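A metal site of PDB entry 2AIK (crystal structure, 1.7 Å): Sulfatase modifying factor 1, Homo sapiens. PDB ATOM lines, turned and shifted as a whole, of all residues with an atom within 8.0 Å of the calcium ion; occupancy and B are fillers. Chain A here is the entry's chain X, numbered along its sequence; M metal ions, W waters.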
ATOM      1  N   TYR A  44     -11.658  17.920 -19.759  1.00  0.00           N
ATOM      2  CA  TYR A  44     -12.823  17.755 -20.600  1.00  0.00           C
ATOM      3  C   TYR A  44     -12.983  18.928 -21.574  1.00  0.00           C
ATOM      4  O   TYR A  44     -12.635  20.070 -21.244  1.00  0.00           O
ATOM      5  CB  TYR A  44     -14.080  17.758 -19.734  1.00  0.00           C
ATOM      6  CG  TYR A  44     -14.020  16.776 -18.572  1.00  0.00           C
ATOM      7  CD1 TYR A  44     -13.997  15.405 -18.807  1.00  0.00           C
ATOM      8  CD2 TYR A  44     -13.908  17.229 -17.258  1.00  0.00           C
ATOM      9  CE1 TYR A  44     -13.950  14.480 -17.754  1.00  0.00           C
ATOM     10  CE2 TYR A  44     -13.860  16.334 -16.208  1.00  0.00           C
ATOM     11  CZ  TYR A  44     -13.868  14.961 -16.449  1.00  0.00           C
ATOM     12  OH  TYR A  44     -13.801  14.075 -15.376  1.00  0.00           O
ATOM     13  N   GLU A  45     -13.570  18.640 -22.740  1.00  0.00           N
ATOM     14  CA  GLU A  45     -14.121  19.698 -23.588  1.00  0.00           C
ATOM     15  C   GLU A  45     -15.081  20.506 -22.704  1.00  0.00           C
ATOM     16  O   GLU A  45     -15.703  19.949 -21.799  1.00  0.00           O
ATOM     17  CB  GLU A  45     -14.893  19.118 -24.757  1.00  0.00           C
ATOM     18  CG  GLU A  45     -14.045  18.332 -25.751  1.00  0.00           C
ATOM     19  CD  GLU A  45     -14.803  17.250 -26.511  1.00  0.00           C
ATOM     20  OE1 GLU A  45     -15.734  16.650 -25.937  1.00  0.00           O
ATOM     21  OE2 GLU A  45     -14.417  16.977 -27.673  1.00  0.00           O
ATOM     22  N   PRO A 120     -20.278  18.344 -25.196  1.00  0.00           N
ATOM     23  CA  PRO A 120     -19.479  19.535 -25.482  1.00  0.00           C
ATOM     24  C   PRO A 120     -20.324  20.644 -26.080  1.00  0.00           C
ATOM     25  O   PRO A 120     -21.210  20.379 -26.879  1.00  0.00           O
ATOM     26  CB  PRO A 120     -18.467  19.054 -26.517  1.00  0.00           C
ATOM     27  CG  PRO A 120     -19.102  17.820 -27.109  1.00  0.00           C
ATOM     28  CD  PRO A 120     -19.811  17.183 -25.968  1.00  0.00           C
ATOM     29  N   TRP A 146      -1.458  21.751 -27.075  1.00  0.00           N
ATOM     30  CA  TRP A 146      -2.589  20.867 -27.350  1.00  0.00           C
ATOM     31  C   TRP A 146      -2.067  19.502 -27.819  1.00  0.00           C
ATOM     32  O   TRP A 146      -2.455  18.446 -27.299  1.00  0.00           O
ATOM     33  CB  TRP A 146      -3.546  21.502 -28.346  1.00  0.00           C
ATOM     34  CG  TRP A 146      -4.835  20.722 -28.506  1.00  0.00           C
ATOM     35  CD1 TRP A 146      -6.057  21.013 -27.948  1.00  0.00           C
ATOM     36  CD2 TRP A 146      -5.002  19.504 -29.232  1.00  0.00           C
ATOM     37  NE1 TRP A 146      -6.971  20.054 -28.323  1.00  0.00           N
ATOM     38  CE2 TRP A 146      -6.344  19.106 -29.078  1.00  0.00           C
ATOM     39  CE3 TRP A 146      -4.140  18.693 -29.994  1.00  0.00           C
ATOM     40  CZ2 TRP A 146      -6.845  17.954 -29.674  1.00  0.00           C
ATOM     41  CZ3 TRP A 146      -4.650  17.533 -30.551  1.00  0.00           C
ATOM     42  CH2 TRP A 146      -5.993  17.173 -30.378  1.00  0.00           C
ATOM     43  N   ASN A 174     -14.928   8.924 -29.892  1.00  0.00           N
ATOM     44  CA  ASN A 174     -16.177   9.085 -30.609  1.00  0.00           C
ATOM     45  C   ASN A 174     -15.896   9.672 -32.007  1.00  0.00           C
ATOM     46  O   ASN A 174     -15.688  10.870 -32.163  1.00  0.00           O
ATOM     47  CB  ASN A 174     -17.157   9.961 -29.846  1.00  0.00           C
ATOM     48  CG  ASN A 174     -18.454  10.149 -30.582  1.00  0.00           C
ATOM     49  OD1 ASN A 174     -18.772   9.348 -31.496  1.00  0.00           O
ATOM     50  ND2 ASN A 174     -19.225  11.180 -30.227  1.00  0.00           N
ATOM     51  N   TYR A 207      -9.860  13.550 -21.617  1.00  0.00           N
ATOM     52  CA  TYR A 207     -10.983  12.853 -22.224  1.00  0.00           C
ATOM     53  C   TYR A 207     -11.305  13.481 -23.581  1.00  0.00           C
ATOM     54  O   TYR A 207     -11.364  14.706 -23.686  1.00  0.00           O
ATOM     55  CB  TYR A 207     -12.224  12.936 -21.332  1.00  0.00           C
ATOM     56  CG  TYR A 207     -12.063  12.173 -20.043  1.00  0.00           C
ATOM     57  CD1 TYR A 207     -11.331  12.713 -18.985  1.00  0.00           C
ATOM     58  CD2 TYR A 207     -12.576  10.875 -19.920  1.00  0.00           C
ATOM     59  CE1 TYR A 207     -11.163  11.998 -17.797  1.00  0.00           C
ATOM     60  CE2 TYR A 207     -12.416  10.150 -18.738  1.00  0.00           C
ATOM     61  CZ  TYR A 207     -11.678  10.713 -17.694  1.00  0.00           C
ATOM     62  OH  TYR A 207     -11.529  10.007 -16.514  1.00  0.00           O
ATOM     63  N   ASN A 208     -11.564  12.641 -24.578  1.00  0.00           N
ATOM     64  CA  ASN A 208     -12.065  13.085 -25.899  1.00  0.00           C
ATOM     65  C   ASN A 208     -11.196  14.122 -26.576  1.00  0.00           C
ATOM     66  O   ASN A 208     -11.683  14.986 -27.309  1.00  0.00           O
ATOM     67  CB  ASN A 208     -13.531  13.546 -25.796  1.00  0.00           C
ATOM     68  CG  ASN A 208     -14.421  12.434 -25.307  1.00  0.00           C
ATOM     69  OD1 ASN A 208     -14.597  11.403 -25.994  1.00  0.00           O
ATOM     70  ND2 ASN A 208     -14.904  12.570 -24.077  1.00  0.00           N
ATOM     71  N   ILE A 209      -9.884  14.015 -26.343  1.00  0.00           N
ATOM     72  CA  ILE A 209      -8.935  14.921 -26.963  1.00  0.00           C
ATOM     73  C   ILE A 209      -8.865  14.668 -28.470  1.00  0.00           C
ATOM     74  O   ILE A 209      -8.743  15.615 -29.247  1.00  0.00           O
ATOM     75  CB  ILE A 209      -7.575  14.907 -26.236  1.00  0.00           C
ATOM     76  CG1 ILE A 209      -6.703  16.050 -26.738  1.00  0.00           C
ATOM     77  CG2 ILE A 209      -6.907  13.601 -26.431  1.00  0.00           C
ATOM     78  CD1 ILE A 209      -7.028  17.330 -26.139  1.00  0.00           C
ATOM     79  N   VAL A 210      -8.978  13.413 -28.911  1.00  0.00           N
ATOM     80  CA  VAL A 210      -9.385  13.156 -30.310  1.00  0.00           C
ATOM     81  C   VAL A 210     -10.863  12.711 -30.365  1.00  0.00           C
ATOM     82  O   VAL A 210     -11.382  12.064 -29.450  1.00  0.00           O
ATOM     83  CB  VAL A 210      -8.490  12.163 -31.052  1.00  0.00           C
ATOM     84  CG1 VAL A 210      -7.084  12.652 -31.081  1.00  0.00           C
ATOM     85  CG2 VAL A 210      -8.525  10.786 -30.456  1.00  0.00           C
ATOM     86  N   GLY A 211     -11.521  13.095 -31.448  1.00  0.00           N
ATOM     87  CA  GLY A 211     -12.950  12.851 -31.637  1.00  0.00           C
ATOM     88  C   GLY A 211     -13.873  13.718 -30.767  1.00  0.00           C
ATOM     89  O   GLY A 211     -13.430  14.640 -30.059  1.00  0.00           O
ATOM     90  N   ASN A 212     -15.165  13.421 -30.887  1.00  0.00           N
ATOM     91  CA  ASN A 212     -16.238  14.144 -30.208  1.00  0.00           C
ATOM     92  C   ASN A 212     -16.405  15.520 -30.852  1.00  0.00           C
ATOM     93  O   ASN A 212     -17.009  15.606 -31.940  1.00  0.00           O
ATOM     94  CB  ASN A 212     -16.080  14.140 -28.676  1.00  0.00           C
ATOM     95  CG  ASN A 212     -17.433  14.057 -27.939  1.00  0.00           C
ATOM     96  OD1 ASN A 212     -18.374  13.419 -28.426  1.00  0.00           O
ATOM     97  ND2 ASN A 212     -17.513  14.656 -26.749  1.00  0.00           N
ATOM     98  N   ALA A 213     -15.893  16.591 -30.246  1.00  0.00           N
ATOM     99  CA  ALA A 213     -15.854  17.889 -30.927  1.00  0.00           C
ATOM    100  C   ALA A 213     -14.399  18.209 -31.327  1.00  0.00           C
ATOM    101  O   ALA A 213     -13.481  17.920 -30.548  1.00  0.00           O
ATOM    102  CB  ALA A 213     -16.362  18.981 -30.007  1.00  0.00           C
ATOM    103  N   TRP A 214     -14.212  18.837 -32.488  1.00  0.00           N
ATOM    104  CA  TRP A 214     -12.966  19.517 -32.833  1.00  0.00           C
ATOM    105  C   TRP A 214     -12.666  20.533 -31.740  1.00  0.00           C
ATOM    106  O   TRP A 214     -13.581  20.986 -31.030  1.00  0.00           O
ATOM    107  CB  TRP A 214     -13.084  20.327 -34.123  1.00  0.00           C
ATOM    108  CG  TRP A 214     -12.867  19.565 -35.383  1.00  0.00           C
ATOM    109  CD1 TRP A 214     -13.820  19.024 -36.177  1.00  0.00           C
ATOM    110  CD2 TRP A 214     -11.617  19.321 -36.020  1.00  0.00           C
ATOM    111  NE1 TRP A 214     -13.231  18.411 -37.278  1.00  0.00           N
ATOM    112  CE2 TRP A 214     -11.877  18.590 -37.199  1.00  0.00           C
ATOM    113  CE3 TRP A 214     -10.288  19.631 -35.694  1.00  0.00           C
ATOM    114  CZ2 TRP A 214     -10.870  18.160 -38.040  1.00  0.00           C
ATOM    115  CZ3 TRP A 214      -9.282  19.210 -36.533  1.00  0.00           C
ATOM    116  CH2 TRP A 214      -9.583  18.482 -37.699  1.00  0.00           C
ATOM    117  N   GLU A 215     -11.399  20.915 -31.603  1.00  0.00           N
ATOM    118  CA  GLU A 215     -11.003  21.869 -30.555  1.00  0.00           C
ATOM    119  C   GLU A 215     -10.141  23.021 -31.060  1.00  0.00           C
ATOM    120  O   GLU A 215      -9.103  22.806 -31.685  1.00  0.00           O
ATOM    121  CB  GLU A 215     -10.290  21.111 -29.449  1.00  0.00           C
ATOM    122  CG  GLU A 215     -11.165  19.956 -28.940  1.00  0.00           C
ATOM    123  CD  GLU A 215     -10.565  19.103 -27.847  1.00  0.00           C
ATOM    124  OE1 GLU A 215      -9.570  19.485 -27.241  1.00  0.00           O
ATOM    125  OE2 GLU A 215     -11.178  18.044 -27.582  1.00  0.00           O
ATOM    126  N   LYS A 245      -7.844  21.286 -33.752  1.00  0.00           N
ATOM    127  CA  LYS A 245      -7.210  19.986 -33.630  1.00  0.00           C
ATOM    128  C   LYS A 245      -8.180  18.911 -33.187  1.00  0.00           C
ATOM    129  O   LYS A 245      -9.206  19.193 -32.528  1.00  0.00           O
ATOM    130  CB  LYS A 245      -6.095  20.043 -32.599  1.00  0.00           C
ATOM    131  CG  LYS A 245      -4.935  21.011 -32.900  1.00  0.00           C
ATOM    132  CD  LYS A 245      -3.945  20.485 -33.933  1.00  0.00           C
ATOM    133  CE  LYS A 245      -2.888  19.579 -33.327  1.00  0.00           C
ATOM    134  NZ  LYS A 245      -1.838  19.198 -34.318  1.00  0.00           N
ATOM    135  N   GLY A 246      -7.825  17.676 -33.528  1.00  0.00           N
ATOM    136  CA  GLY A 246      -8.350  16.505 -32.864  1.00  0.00           C
ATOM    137  C   GLY A 246      -9.463  15.716 -33.522  1.00  0.00           C
ATOM    138  O   GLY A 246      -9.770  14.581 -33.081  1.00  0.00           O
ATOM    139  N   GLY A 247     -10.097  16.298 -34.546  1.00  0.00           N
ATOM    140  CA  GLY A 247     -11.211  15.654 -35.217  1.00  0.00           C
ATOM    141  C   GLY A 247     -12.429  15.594 -34.311  1.00  0.00           C
ATOM    142  O   GLY A 247     -12.440  16.179 -33.227  1.00  0.00           O
ATOM    143  N   SER A 248     -13.464  14.923 -34.810  1.00  0.00           N
ATOM    144  CA  SER A 248     -14.798  14.974 -34.250  1.00  0.00           C
ATOM    145  C   SER A 248     -15.549  13.672 -34.447  1.00  0.00           C
ATOM    146  O   SER A 248     -15.066  12.726 -35.081  1.00  0.00           O
ATOM    147  CB  SER A 248     -15.621  16.097 -34.913  1.00  0.00           C
ATOM    148  OG  SER A 248     -16.146  15.711 -36.185  1.00  0.00           O
ATOM    149  N   TYR A 249     -16.756  13.651 -33.906  1.00  0.00           N
ATOM    150  CA  TYR A 249     -17.676  12.534 -34.125  1.00  0.00           C
ATOM    151  C   TYR A 249     -17.967  12.205 -35.607  1.00  0.00           C
ATOM    152  O   TYR A 249     -18.514  11.126 -35.934  1.00  0.00           O
ATOM    153  CB  TYR A 249     -18.970  12.804 -33.367  1.00  0.00           C
ATOM    154  CG  TYR A 249     -19.899  13.855 -33.930  1.00  0.00           C
ATOM    155  CD1 TYR A 249     -19.947  15.141 -33.381  1.00  0.00           C
ATOM    156  CD2 TYR A 249     -20.776  13.544 -34.953  1.00  0.00           C
ATOM    157  CE1 TYR A 249     -20.856  16.094 -33.887  1.00  0.00           C
ATOM    158  CE2 TYR A 249     -21.650  14.471 -35.458  1.00  0.00           C
ATOM    159  CZ  TYR A 249     -21.707  15.730 -34.933  1.00  0.00           C
ATOM    160  OH  TYR A 249     -22.608  16.662 -35.428  1.00  0.00           O
ATOM    161  N   ASN A 275     -19.767  20.598 -35.157  1.00  0.00           N
ATOM    162  CA  ASN A 275     -18.747  19.619 -34.772  1.00  0.00           C
ATOM    163  C   ASN A 275     -17.521  20.244 -34.139  1.00  0.00           C
ATOM    164  O   ASN A 275     -16.467  19.581 -34.043  1.00  0.00           O
ATOM    165  CB  ASN A 275     -18.343  18.760 -35.968  1.00  0.00           C
ATOM    166  CG  ASN A 275     -17.548  19.537 -37.009  1.00  0.00           C
ATOM    167  OD1 ASN A 275     -17.500  20.762 -36.954  1.00  0.00           O
ATOM    168  ND2 ASN A 275     -16.877  18.807 -37.933  1.00  0.00           N
ATOM    169  N   GLY A 277     -15.863  22.634 -30.951  1.00  0.00           N
ATOM    170  CA  GLY A 277     -15.873  23.147 -29.607  1.00  0.00           C
ATOM    171  C   GLY A 277     -14.455  23.515 -29.175  1.00  0.00           C
ATOM    172  O   GLY A 277     -13.639  23.983 -29.989  1.00  0.00           O
ATOM    173  N   PHE A 278     -14.177  23.290 -27.886  1.00  0.00           N
ATOM    174  CA  PHE A 278     -12.881  23.680 -27.316  1.00  0.00           C
ATOM    175  C   PHE A 278     -12.726  23.230 -25.878  1.00  0.00           C
ATOM    176  O   PHE A 278     -13.715  22.874 -25.221  1.00  0.00           O
ATOM    177  CB  PHE A 278     -12.681  25.208 -27.366  1.00  0.00           C
ATOM    178  CG  PHE A 278     -13.589  25.988 -26.450  1.00  0.00           C
ATOM    179  CD1 PHE A 278     -13.096  26.525 -25.263  1.00  0.00           C
ATOM    180  CD2 PHE A 278     -14.916  26.189 -26.772  1.00  0.00           C
ATOM    181  CE1 PHE A 278     -13.918  27.257 -24.417  1.00  0.00           C
ATOM    182  CE2 PHE A 278     -15.758  26.894 -25.908  1.00  0.00           C
ATOM    183  CZ  PHE A 278     -15.252  27.444 -24.724  1.00  0.00           C
ATOM    184  N   ARG A 279     -11.483  23.311 -25.408  1.00  0.00           N
ATOM    185  CA  ARG A 279     -11.137  23.190 -24.002  1.00  0.00           C
ATOM    186  C   ARG A 279     -10.108  24.274 -23.665  1.00  0.00           C
ATOM    187  O   ARG A 279      -9.453  24.815 -24.568  1.00  0.00           O
ATOM    188  CB  ARG A 279     -10.601  21.823 -23.670  1.00  0.00           C
ATOM    189  CG  ARG A 279      -9.161  21.536 -24.126  1.00  0.00           C
ATOM    190  CD  ARG A 279      -8.684  20.105 -23.759  1.00  0.00           C
ATOM    191  NE  ARG A 279      -9.416  19.101 -24.534  1.00  0.00           N
ATOM    192  CZ  ARG A 279      -9.897  17.947 -24.061  1.00  0.00           C
ATOM    193  NH1 ARG A 279      -9.796  17.597 -22.789  1.00  0.00           N
ATOM    194  NH2 ARG A 279     -10.552  17.148 -24.897  1.00  0.00           N
HETATM  195 CA    CA M   1     -12.477  16.555 -28.902  1.00  0.00          CA
HETATM  196  O   HOH W   1     -10.928  16.536 -30.632  1.00  0.00           O
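The side-chain carboxylate (OE1) of Glu 45 lies within hydrogen-bond range of the side-chain amide nitrogen (ND2) of Asn 212 (2.8 Å).
The guanidinium group of Arg 279 sits close to the backbone carbonyl oxygen of Asn 208 (3.4 Å).
The side-chain carboxylate (OE1) of Glu 215 lies within salt-bridge range of the guanidinium group (NE) of Arg 279 (2.7 Å).
N of Lys 245 sits at hydrogen-bond distance from O of Glu 215, at 2.9 Å.
The side-chain carboxylate (OE1) of Glu 215 sits at hydrogen-bond distance from the indole nitrogen (NE1) of Trp 146, 2.9 Å away.
The backbone carbonyl oxygen (O) of Gly 246 is in hydrogen-bond range of the backbone NH (N) of Gly 211.
Residues that only touch the calcium ion: Ile 209 (3.9 Å).
The calcium ion is bound by water W1 (2.3 Å), OE2 of Glu 45 (2.3 Å), O of Ala 213 (2.4 Å), O of Asn 208 (2.4 Å), OE2 of Glu 215 (2.4 Å) and O of Gly 211 (2.4 Å).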
